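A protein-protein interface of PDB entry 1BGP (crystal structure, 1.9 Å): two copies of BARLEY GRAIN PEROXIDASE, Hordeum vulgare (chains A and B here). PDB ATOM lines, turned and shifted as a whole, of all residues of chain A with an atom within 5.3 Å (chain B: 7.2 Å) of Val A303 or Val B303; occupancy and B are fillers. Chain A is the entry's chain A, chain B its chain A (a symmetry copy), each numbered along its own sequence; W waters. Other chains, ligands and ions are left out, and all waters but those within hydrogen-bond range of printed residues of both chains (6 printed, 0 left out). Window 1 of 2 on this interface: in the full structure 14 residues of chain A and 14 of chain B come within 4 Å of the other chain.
Asp A63 touches Val B303, and with the chains exchanged Val A303 touches Asp B63. Asp A63 touches Arg B304, and with the chains exchanged Arg A304 touches Asp B63. Val A303 touches its own counterpart, Val B303.
Of the printed residues of chain B, Val A303 touches Asp B63 and Val B303. Of chain A, only Asp A63 (3.5 Å) and Val A303 (3.3 Å) come within 4 Å of Val B303. Of the printed residues of chain A, Phe B138 touches Asp A63. Of the printed residues of chain A, Arg B304 touches Asp A63 (3.0 Å). Of the printed residues of chain B, Asp A63 touches Phe B138 (3.4 Å), Val B303 (3.5 Å) and Arg B304 (3.0 Å). Of the printed residues of chain B, Arg A304 touches Asp B63. Of the printed residues of chain A, Asp B63 touches Val A303 (3.5 Å) and Arg A304 (3.0 Å). Glu B296 touches none of the printed residues of chain A. The nearest printed residue of chain A that does not touch Asp B63 is Ser A302 (4.5 Å).
The guanidinium group (NE) of Arg A304 lies within salt-bridge range of the side-chain carboxylate (OD1) of Asp B63 (3.2 Å). The side-chain carboxylate of Asp A63 lies within salt-bridge range of the guanidinium group of Arg B304 (3.2 Å).
Of the 21 printed residues of chain B, 4 touch a printed residue of chain A. Hydrophobic or aromatic side chains of chain B within 4 Å of the printed part of chain A: Phe B138 and Val B303. Among the printed residues, 6 pairs touch across the chains.
The backbone NH of Asp A63 is in hydrogen-bond range of the backbone carbonyl oxygen of Ser A302. N of Asp B63 is in hydrogen-bond range of O of Ser B302. The side-chain sulfur of Cys B106 forms a disulfide with the side-chain sulfur of Cys B301. O of Arg B136 lies close to NH1 of Arg B304 (3.4 Å).
Water W4 lies within hydrogen-bond range of O of Ser A302, OD2 of Asp B63 and N of Asp A63. Water W6 lies within hydrogen-bond range of O of Ser B302, OD2 of Asp A63, N of Asp B63 and N of Gly B64. Water W3 lies within hydrogen-bond range of O of Asp A63 and NH2 of Arg B304. Water W1 lies within hydrogen-bond range of O of Asp B63 (2.6 Å) and NH2 of Arg A304 (3.1 Å). Water W5 bridges O of Arg B304 (2.8 Å) and OD1 of Asp A63 (2.9 Å). Water W2 lies within hydrogen-bond range of O of Arg A304 and OD1 of Asp B63.
Asp A63 touches Phe B138 (O to CZ, 3.4 Å). OD2 of Asp A63 touches CA of Val B303, at 3.5 Å. Asp B63 touches Val A303. Val B303 touches Val A303.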
ATOM      1  N   LEU A  62       9.341 -25.800 -36.202  1.00  0.00           N
ATOM      2  CA  LEU A  62       8.889 -25.170 -34.969  1.00  0.00           C
ATOM      3  C   LEU A  62       7.887 -24.056 -35.228  1.00  0.00           C
ATOM      4  O   LEU A  62       8.100 -23.195 -36.090  1.00  0.00           O
ATOM      5  CB  LEU A  62      10.082 -24.602 -34.197  1.00  0.00           C
ATOM      6  CG  LEU A  62      11.115 -25.602 -33.671  1.00  0.00           C
ATOM      7  CD1 LEU A  62      12.319 -24.851 -33.150  1.00  0.00           C
ATOM      8  CD2 LEU A  62      10.503 -26.472 -32.580  1.00  0.00           C
ATOM      9  N   ASP A  63       6.812 -24.054 -34.447  1.00  0.00           N
ATOM     10  CA  ASP A  63       5.771 -23.040 -34.565  1.00  0.00           C
ATOM     11  C   ASP A  63       6.362 -21.651 -34.313  1.00  0.00           C
ATOM     12  O   ASP A  63       5.951 -20.670 -34.926  1.00  0.00           O
ATOM     13  CB  ASP A  63       4.635 -23.335 -33.576  1.00  0.00           C
ATOM     14  CG  ASP A  63       3.528 -22.292 -33.617  1.00  0.00           C
ATOM     15  OD1 ASP A  63       3.042 -21.965 -34.721  1.00  0.00           O
ATOM     16  OD2 ASP A  63       3.140 -21.801 -32.538  1.00  0.00           O
ATOM     17  N   GLU A 296      18.489 -31.785 -29.660  1.00  0.00           N
ATOM     18  CA  GLU A 296      17.675 -32.751 -28.945  1.00  0.00           C
ATOM     19  C   GLU A 296      16.835 -33.558 -29.916  1.00  0.00           C
ATOM     20  O   GLU A 296      16.889 -33.349 -31.129  1.00  0.00           O
ATOM     21  CB  GLU A 296      16.757 -32.028 -27.952  1.00  0.00           C
ATOM     22  CG  GLU A 296      15.798 -31.035 -28.609  1.00  0.00           C
ATOM     23  CD  GLU A 296      14.904 -30.311 -27.614  1.00  0.00           C
ATOM     24  OE1 GLU A 296      15.273 -30.214 -26.424  1.00  0.00           O
ATOM     25  OE2 GLU A 296      13.832 -29.829 -28.027  1.00  0.00           O
ATOM     26  N   ARG A 298      13.132 -34.160 -30.512  1.00  0.00           N
ATOM     27  CA  ARG A 298      11.795 -33.680 -30.180  1.00  0.00           C
ATOM     28  C   ARG A 298      10.746 -34.761 -30.020  1.00  0.00           C
ATOM     29  O   ARG A 298      10.736 -35.753 -30.754  1.00  0.00           O
ATOM     30  CB  ARG A 298      11.312 -32.674 -31.222  1.00  0.00           C
ATOM     31  CG  ARG A 298      12.166 -31.442 -31.333  1.00  0.00           C
ATOM     32  CD  ARG A 298      11.586 -30.489 -32.348  1.00  0.00           C
ATOM     33  NE  ARG A 298      12.559 -29.475 -32.736  1.00  0.00           N
ATOM     34  CZ  ARG A 298      12.589 -28.881 -33.923  1.00  0.00           C
ATOM     35  NH1 ARG A 298      11.691 -29.190 -34.852  1.00  0.00           N
ATOM     36  NH2 ARG A 298      13.536 -27.993 -34.190  1.00  0.00           N
ATOM     37  N   ASN A 300       7.749 -33.829 -30.212  1.00  0.00           N
ATOM     38  CA  ASN A 300       6.757 -33.212 -31.088  1.00  0.00           C
ATOM     39  C   ASN A 300       7.566 -32.230 -31.916  1.00  0.00           C
ATOM     40  O   ASN A 300       8.164 -31.307 -31.368  1.00  0.00           O
ATOM     41  CB  ASN A 300       5.697 -32.460 -30.283  1.00  0.00           C
ATOM     42  CG  ASN A 300       4.650 -31.807 -31.170  1.00  0.00           C
ATOM     43  OD1 ASN A 300       4.975 -31.092 -32.119  1.00  0.00           O
ATOM     44  ND2 ASN A 300       3.386 -32.049 -30.864  1.00  0.00           N
ATOM     45  N   CYS A 301       7.576 -32.415 -33.231  1.00  0.00           N
ATOM     46  CA  CYS A 301       8.363 -31.558 -34.115  1.00  0.00           C
ATOM     47  C   CYS A 301       8.038 -30.065 -34.112  1.00  0.00           C
ATOM     48  O   CYS A 301       8.898 -29.245 -34.437  1.00  0.00           O
ATOM     49  CB  CYS A 301       8.336 -32.107 -35.542  1.00  0.00           C
ATOM     50  SG  CYS A 301       8.953 -33.815 -35.671  1.00  0.00           S
ATOM     51  N   SER A 302       6.813 -29.713 -33.729  1.00  0.00           N
ATOM     52  CA  SER A 302       6.386 -28.314 -33.705  1.00  0.00           C
ATOM     53  C   SER A 302       6.893 -27.510 -32.518  1.00  0.00           C
ATOM     54  O   SER A 302       6.894 -26.277 -32.557  1.00  0.00           O
ATOM     55  CB  SER A 302       4.860 -28.226 -33.740  1.00  0.00           C
ATOM     56  OG  SER A 302       4.338 -28.906 -34.866  1.00  0.00           O
ATOM     57  N   VAL A 303       7.308 -28.194 -31.458  1.00  0.00           N
ATOM     58  CA  VAL A 303       7.790 -27.503 -30.269  1.00  0.00           C
ATOM     59  C   VAL A 303       9.065 -28.084 -29.699  1.00  0.00           C
ATOM     60  O   VAL A 303       9.392 -29.251 -29.912  1.00  0.00           O
ATOM     61  CB  VAL A 303       6.745 -27.523 -29.122  1.00  0.00           C
ATOM     62  CG1 VAL A 303       5.522 -26.726 -29.500  1.00  0.00           C
ATOM     63  CG2 VAL A 303       6.374 -28.957 -28.768  1.00  0.00           C
ATOM     64  N   ARG A 304       9.773 -27.250 -28.952  1.00  0.00           N
ATOM     65  CA  ARG A 304      10.989 -27.673 -28.293  1.00  0.00           C
ATOM     66  C   ARG A 304      10.518 -28.469 -27.084  1.00  0.00           C
ATOM     67  O   ARG A 304       9.410 -28.249 -26.578  1.00  0.00           O
ATOM     68  CB  ARG A 304      11.788 -26.452 -27.852  1.00  0.00           C
ATOM     69  CG  ARG A 304      12.172 -25.558 -29.010  1.00  0.00           C
ATOM     70  CD  ARG A 304      12.773 -24.266 -28.537  1.00  0.00           C
ATOM     71  NE  ARG A 304      11.808 -23.439 -27.823  1.00  0.00           N
ATOM     72  CZ  ARG A 304      12.137 -22.372 -27.104  1.00  0.00           C
ATOM     73  NH1 ARG A 304      13.408 -22.005 -27.009  1.00  0.00           N
ATOM     74  NH2 ARG A 304      11.197 -21.670 -26.488  1.00  0.00           N
ATOM     75  N   ASN A 305      11.317 -29.439 -26.662  1.00  0.00           N
ATOM     76  CA  ASN A 305      10.962 -30.249 -25.508  1.00  0.00           C
ATOM     77  C   ASN A 305      10.853 -29.321 -24.307  1.00  0.00           C
ATOM     78  O   ASN A 305      11.780 -28.566 -24.008  1.00  0.00           O
ATOM     79  CB  ASN A 305      12.014 -31.338 -25.269  1.00  0.00           C
ATOM     80  CG  ASN A 305      11.997 -32.409 -26.344  1.00  0.00           C
ATOM     81  OD1 ASN A 305      11.025 -32.539 -27.092  1.00  0.00           O
ATOM     82  ND2 ASN A 305      13.066 -33.187 -26.421  1.00  0.00           N
ATOM     83  N   LEU B  61       1.693 -19.440 -22.963  1.00  0.00           N
ATOM     84  CA  LEU B  61       1.595 -20.895 -23.029  1.00  0.00           C
ATOM     85  C   LEU B  61       2.287 -21.391 -24.298  1.00  0.00           C
ATOM     86  O   LEU B  61       2.664 -22.561 -24.397  1.00  0.00           O
ATOM     87  CB  LEU B  61       0.131 -21.352 -23.039  1.00  0.00           C
ATOM     88  CG  LEU B  61      -0.756 -20.995 -21.844  1.00  0.00           C
ATOM     89  CD1 LEU B  61      -2.063 -21.762 -21.949  1.00  0.00           C
ATOM     90  CD2 LEU B  61      -0.051 -21.338 -20.538  1.00  0.00           C
ATOM     91  N   LEU B  62       2.434 -20.488 -25.264  1.00  0.00           N
ATOM     92  CA  LEU B  62       3.062 -20.799 -26.541  1.00  0.00           C
ATOM     93  C   LEU B  62       4.562 -21.007 -26.408  1.00  0.00           C
ATOM     94  O   LEU B  62       5.262 -20.208 -25.775  1.00  0.00           O
ATOM     95  CB  LEU B  62       2.799 -19.676 -27.547  1.00  0.00           C
ATOM     96  CG  LEU B  62       1.346 -19.439 -27.968  1.00  0.00           C
ATOM     97  CD1 LEU B  62       1.259 -18.160 -28.769  1.00  0.00           C
ATOM     98  CD2 LEU B  62       0.828 -20.623 -28.775  1.00  0.00           C
ATOM     99  N   ASP B  63       5.057 -22.065 -27.043  1.00  0.00           N
ATOM    100  CA  ASP B  63       6.478 -22.386 -27.020  1.00  0.00           C
ATOM    101  C   ASP B  63       7.285 -21.234 -27.624  1.00  0.00           C
ATOM    102  O   ASP B  63       8.396 -20.945 -27.187  1.00  0.00           O
ATOM    103  CB  ASP B  63       6.734 -23.690 -27.789  1.00  0.00           C
ATOM    104  CG  ASP B  63       8.207 -24.068 -27.840  1.00  0.00           C
ATOM    105  OD1 ASP B  63       8.870 -24.073 -26.779  1.00  0.00           O
ATOM    106  OD2 ASP B  63       8.702 -24.364 -28.946  1.00  0.00           O
ATOM    107  N   GLY B  64       6.700 -20.550 -28.601  1.00  0.00           N
ATOM    108  CA  GLY B  64       7.390 -19.446 -29.239  1.00  0.00           C
ATOM    109  C   GLY B  64       7.492 -18.192 -28.393  1.00  0.00           C
ATOM    110  O   GLY B  64       8.196 -17.257 -28.763  1.00  0.00           O
ATOM    111  N   PRO B  69       6.832 -22.417 -22.159  1.00  0.00           N
ATOM    112  CA  PRO B  69       7.191 -23.788 -21.791  1.00  0.00           C
ATOM    113  C   PRO B  69       8.577 -24.287 -22.195  1.00  0.00           C
ATOM    114  O   PRO B  69       9.137 -25.152 -21.520  1.00  0.00           O
ATOM    115  CB  PRO B  69       6.079 -24.615 -22.434  1.00  0.00           C
ATOM    116  CG  PRO B  69       5.694 -23.795 -23.620  1.00  0.00           C
ATOM    117  CD  PRO B  69       5.650 -22.415 -23.037  1.00  0.00           C
ATOM    118  N   ASN B  89      -2.420 -28.106 -20.522  1.00  0.00           N
ATOM    119  CA  ASN B  89      -2.549 -28.904 -21.741  1.00  0.00           C
ATOM    120  C   ASN B  89      -3.430 -30.118 -21.493  1.00  0.00           C
ATOM    121  O   ASN B  89      -4.302 -30.433 -22.305  1.00  0.00           O
ATOM    122  CB  ASN B  89      -1.180 -29.349 -22.265  1.00  0.00           C
ATOM    123  CG  ASN B  89      -0.436 -28.237 -22.983  1.00  0.00           C
ATOM    124  OD1 ASN B  89      -1.036 -27.432 -23.697  1.00  0.00           O
ATOM    125  ND2 ASN B  89       0.877 -28.188 -22.802  1.00  0.00           N
ATOM    126  N   CYS B 106      -7.683 -21.910 -24.300  1.00  0.00           N
ATOM    127  CA  CYS B 106      -6.664 -22.105 -23.273  1.00  0.00           C
ATOM    128  C   CYS B 106      -6.697 -20.919 -22.306  1.00  0.00           C
ATOM    129  O   CYS B 106      -6.414 -21.073 -21.116  1.00  0.00           O
ATOM    130  CB  CYS B 106      -5.274 -22.232 -23.914  1.00  0.00           C
ATOM    131  SG  CYS B 106      -5.114 -23.615 -25.094  1.00  0.00           S
ATOM    132  N   ASP B 134      -7.704 -17.288 -27.687  1.00  0.00           N
ATOM    133  CA  ASP B 134      -6.256 -17.460 -27.619  1.00  0.00           C
ATOM    134  C   ASP B 134      -5.533 -16.626 -28.659  1.00  0.00           C
ATOM    135  O   ASP B 134      -5.951 -16.555 -29.817  1.00  0.00           O
ATOM    136  CB  ASP B 134      -5.891 -18.933 -27.783  1.00  0.00           C
ATOM    137  CG  ASP B 134      -6.509 -19.799 -26.714  1.00  0.00           C
ATOM    138  OD1 ASP B 134      -6.630 -19.323 -25.568  1.00  0.00           O
ATOM    139  OD2 ASP B 134      -6.875 -20.954 -27.015  1.00  0.00           O
ATOM    140  N   SER B 135      -4.443 -16.003 -28.238  1.00  0.00           N
ATOM    141  CA  SER B 135      -3.651 -15.157 -29.115  1.00  0.00           C
ATOM    142  C   SER B 135      -2.750 -15.957 -30.054  1.00  0.00           C
ATOM    143  O   SER B 135      -2.326 -17.071 -29.731  1.00  0.00           O
ATOM    144  CB  SER B 135      -2.793 -14.207 -28.281  1.00  0.00           C
ATOM    145  OG  SER B 135      -2.028 -13.349 -29.108  1.00  0.00           O
ATOM    146  N   ARG B 136      -2.488 -15.386 -31.225  1.00  0.00           N
ATOM    147  CA  ARG B 136      -1.608 -15.993 -32.214  1.00  0.00           C
ATOM    148  C   ARG B 136      -0.308 -15.195 -32.234  1.00  0.00           C
ATOM    149  O   ARG B 136       0.525 -15.360 -33.130  1.00  0.00           O
ATOM    150  CB  ARG B 136      -2.243 -15.973 -33.608  1.00  0.00           C
ATOM    151  CG  ARG B 136      -3.366 -16.967 -33.804  1.00  0.00           C
ATOM    152  CD  ARG B 136      -3.724 -17.101 -35.283  1.00  0.00           C
ATOM    153  NE  ARG B 136      -2.592 -17.597 -36.069  1.00  0.00           N
ATOM    154  CZ  ARG B 136      -2.378 -18.878 -36.359  1.00  0.00           C
ATOM    155  NH1 ARG B 136      -3.217 -19.810 -35.935  1.00  0.00           N
ATOM    156  NH2 ARG B 136      -1.313 -19.232 -37.066  1.00  0.00           N
ATOM    157  N   PHE B 138       3.196 -14.186 -30.316  1.00  0.00           N
ATOM    158  CA  PHE B 138       4.157 -14.636 -29.318  1.00  0.00           C
ATOM    159  C   PHE B 138       4.577 -13.445 -28.465  1.00  0.00           C
ATOM    160  O   PHE B 138       4.577 -12.298 -28.929  1.00  0.00           O
ATOM    161  CB  PHE B 138       5.410 -15.218 -29.985  1.00  0.00           C
ATOM    162  CG  PHE B 138       5.154 -16.440 -30.818  1.00  0.00           C
ATOM    163  CD1 PHE B 138       4.457 -17.526 -30.296  1.00  0.00           C
ATOM    164  CD2 PHE B 138       5.619 -16.508 -32.129  1.00  0.00           C
ATOM    165  CE1 PHE B 138       4.227 -18.661 -31.066  1.00  0.00           C
ATOM    166  CE2 PHE B 138       5.393 -17.641 -32.910  1.00  0.00           C
ATOM    167  CZ  PHE B 138       4.697 -18.718 -32.376  1.00  0.00           C
ATOM    168  N   GLU B 296      -8.259 -17.312 -31.418  1.00  0.00           N
ATOM    169  CA  GLU B 296      -8.705 -18.635 -31.817  1.00  0.00           C
ATOM    170  C   GLU B 296      -8.809 -19.545 -30.608  1.00  0.00           C
ATOM    171  O   GLU B 296      -8.525 -19.139 -29.480  1.00  0.00           O
ATOM    172  CB  GLU B 296      -7.720 -19.236 -32.826  1.00  0.00           C
ATOM    173  CG  GLU B 296      -6.297 -19.387 -32.285  1.00  0.00           C
ATOM    174  CD  GLU B 296      -5.324 -19.967 -33.301  1.00  0.00           C
ATOM    175  OE1 GLU B 296      -5.581 -19.860 -34.519  1.00  0.00           O
ATOM    176  OE2 GLU B 296      -4.295 -20.527 -32.877  1.00  0.00           O
ATOM    177  N   ARG B 298      -7.234 -22.812 -29.478  1.00  0.00           N
ATOM    178  CA  ARG B 298      -6.148 -23.748 -29.746  1.00  0.00           C
ATOM    179  C   ARG B 298      -6.499 -25.209 -29.555  1.00  0.00           C
ATOM    180  O   ARG B 298      -7.235 -25.573 -28.633  1.00  0.00           O
ATOM    181  CB  ARG B 298      -4.929 -23.416 -28.889  1.00  0.00           C
ATOM    182  CG  ARG B 298      -4.354 -22.049 -29.138  1.00  0.00           C
ATOM    183  CD  ARG B 298      -3.129 -21.831 -28.284  1.00  0.00           C
ATOM    184  NE  ARG B 298      -2.768 -20.420 -28.231  1.00  0.00           N
ATOM    185  CZ  ARG B 298      -2.153 -19.841 -27.206  1.00  0.00           C
ATOM    186  NH1 ARG B 298      -1.817 -20.553 -26.137  1.00  0.00           N
ATOM    187  NH2 ARG B 298      -1.897 -18.542 -27.243  1.00  0.00           N
ATOM    188  N   ARG B 299      -5.971 -26.041 -30.448  1.00  0.00           N
ATOM    189  CA  ARG B 299      -6.170 -27.482 -30.389  1.00  0.00           C
ATOM    190  C   ARG B 299      -5.038 -28.050 -29.532  1.00  0.00           C
ATOM    191  O   ARG B 299      -5.013 -29.238 -29.213  1.00  0.00           O
ATOM    192  CB  ARG B 299      -6.126 -28.089 -31.794  1.00  0.00           C
ATOM    193  CG  ARG B 299      -7.062 -27.425 -32.786  1.00  0.00           C
ATOM    194  CD  ARG B 299      -6.880 -28.012 -34.172  1.00  0.00           C
ATOM    195  NE  ARG B 299      -7.326 -27.091 -35.216  1.00  0.00           N
ATOM    196  CZ  ARG B 299      -6.658 -26.856 -36.344  1.00  0.00           C
ATOM    197  NH1 ARG B 299      -5.506 -27.474 -36.589  1.00  0.00           N
ATOM    198  NH2 ARG B 299      -7.131 -25.982 -37.223  1.00  0.00           N
ATOM    199  N   ASN B 300      -4.076 -27.186 -29.218  1.00  0.00           N
ATOM    200  CA  ASN B 300      -2.924 -27.512 -28.382  1.00  0.00           C
ATOM    201  C   ASN B 300      -2.449 -26.161 -27.877  1.00  0.00           C
ATOM    202  O   ASN B 300      -2.069 -25.304 -28.671  1.00  0.00           O
ATOM    203  CB  ASN B 300      -1.816 -28.177 -29.199  1.00  0.00           C
ATOM    204  CG  ASN B 300      -0.603 -28.527 -28.354  1.00  0.00           C
ATOM    205  OD1 ASN B 300      -0.075 -27.692 -27.619  1.00  0.00           O
ATOM    206  ND2 ASN B 300      -0.154 -29.768 -28.455  1.00  0.00           N
ATOM    207  N   CYS B 301      -2.458 -25.973 -26.562  1.00  0.00           N
ATOM    208  CA  CYS B 301      -2.069 -24.693 -25.974  1.00  0.00           C
ATOM    209  C   CYS B 301      -0.651 -24.198 -26.252  1.00  0.00           C
ATOM    210  O   CYS B 301      -0.396 -22.994 -26.207  1.00  0.00           O
ATOM    211  CB  CYS B 301      -2.347 -24.699 -24.470  1.00  0.00           C
ATOM    212  SG  CYS B 301      -4.089 -25.035 -24.059  1.00  0.00           S
ATOM    213  N   SER B 302       0.263 -25.117 -26.556  1.00  0.00           N
ATOM    214  CA  SER B 302       1.656 -24.760 -26.824  1.00  0.00           C
ATOM    215  C   SER B 302       1.913 -24.173 -28.202  1.00  0.00           C
ATOM    216  O   SER B 302       2.944 -23.533 -28.422  1.00  0.00           O
ATOM    217  CB  SER B 302       2.560 -25.978 -26.632  1.00  0.00           C
ATOM    218  OG  SER B 302       2.406 -26.526 -25.336  1.00  0.00           O
ATOM    219  N   VAL B 303       0.997 -24.401 -29.137  1.00  0.00           N
ATOM    220  CA  VAL B 303       1.174 -23.895 -30.491  1.00  0.00           C
ATOM    221  C   VAL B 303      -0.065 -23.250 -31.070  1.00  0.00           C
ATOM    222  O   VAL B 303      -1.190 -23.532 -30.657  1.00  0.00           O
ATOM    223  CB  VAL B 303       1.592 -25.014 -31.480  1.00  0.00           C
ATOM    224  CG1 VAL B 303       2.962 -25.544 -31.139  1.00  0.00           C
ATOM    225  CG2 VAL B 303       0.559 -26.133 -31.482  1.00  0.00           C
ATOM    226  N   ARG B 304       0.158 -22.389 -32.051  1.00  0.00           N
ATOM    227  CA  ARG B 304      -0.929 -21.731 -32.743  1.00  0.00           C
ATOM    228  C   ARG B 304      -1.475 -22.785 -33.696  1.00  0.00           C
ATOM    229  O   ARG B 304      -0.750 -23.700 -34.105  1.00  0.00           O
ATOM    230  CB  ARG B 304      -0.396 -20.533 -33.518  1.00  0.00           C
ATOM    231  CG  ARG B 304       0.274 -19.512 -32.625  1.00  0.00           C
ATOM    232  CD  ARG B 304       0.969 -18.447 -33.423  1.00  0.00           C
ATOM    233  NE  ARG B 304       2.098 -18.976 -34.179  1.00  0.00           N
ATOM    234  CZ  ARG B 304       2.725 -18.305 -35.138  1.00  0.00           C
ATOM    235  NH1 ARG B 304       2.331 -17.078 -35.454  1.00  0.00           N
ATOM    236  NH2 ARG B 304       3.748 -18.856 -35.775  1.00  0.00           N
ATOM    237  N   ASN B 305      -2.764 -22.706 -33.994  1.00  0.00           N
ATOM    238  CA  ASN B 305      -3.378 -23.658 -34.905  1.00  0.00           C
ATOM    239  C   ASN B 305      -2.685 -23.524 -36.253  1.00  0.00           C
ATOM    240  O   ASN B 305      -2.594 -22.428 -36.808  1.00  0.00           O
ATOM    241  CB  ASN B 305      -4.883 -23.392 -35.031  1.00  0.00           C
ATOM    242  CG  ASN B 305      -5.641 -23.730 -33.761  1.00  0.00           C
ATOM    243  OD1 ASN B 305      -5.137 -24.450 -32.894  1.00  0.00           O
ATOM    244  ND2 ASN B 305      -6.860 -23.223 -33.645  1.00  0.00           N
ATOM    245  N   PRO B 306      -2.111 -24.626 -36.756  1.00  0.00           N
ATOM    246  CA  PRO B 306      -1.419 -24.589 -38.045  1.00  0.00           C
ATOM    247  C   PRO B 306      -2.381 -24.312 -39.194  1.00  0.00           C
ATOM    248  O   PRO B 306      -3.588 -24.532 -39.071  1.00  0.00           O
ATOM    249  CB  PRO B 306      -0.805 -25.984 -38.136  1.00  0.00           C
ATOM    250  CG  PRO B 306      -1.791 -26.831 -37.403  1.00  0.00           C
ATOM    251  CD  PRO B 306      -2.099 -25.986 -36.190  1.00  0.00           C
HETATM  252  O   HOH W   1       8.863 -20.955 -24.605  1.00  0.00           O
HETATM  253  O   HOH W   2       7.840 -26.350 -25.310  1.00  0.00           O
HETATM  254  O   HOH W   3       5.392 -20.826 -37.484  1.00  0.00           O
HETATM  255  O   HOH W   4       7.552 -23.967 -31.540  1.00  0.00           O
HETATM  256  O   HOH W   5       1.536 -24.298 -35.553  1.00  0.00           O
HETATM  257  O   HOH W   6       4.393 -22.012 -29.969  1.00  0.00           O
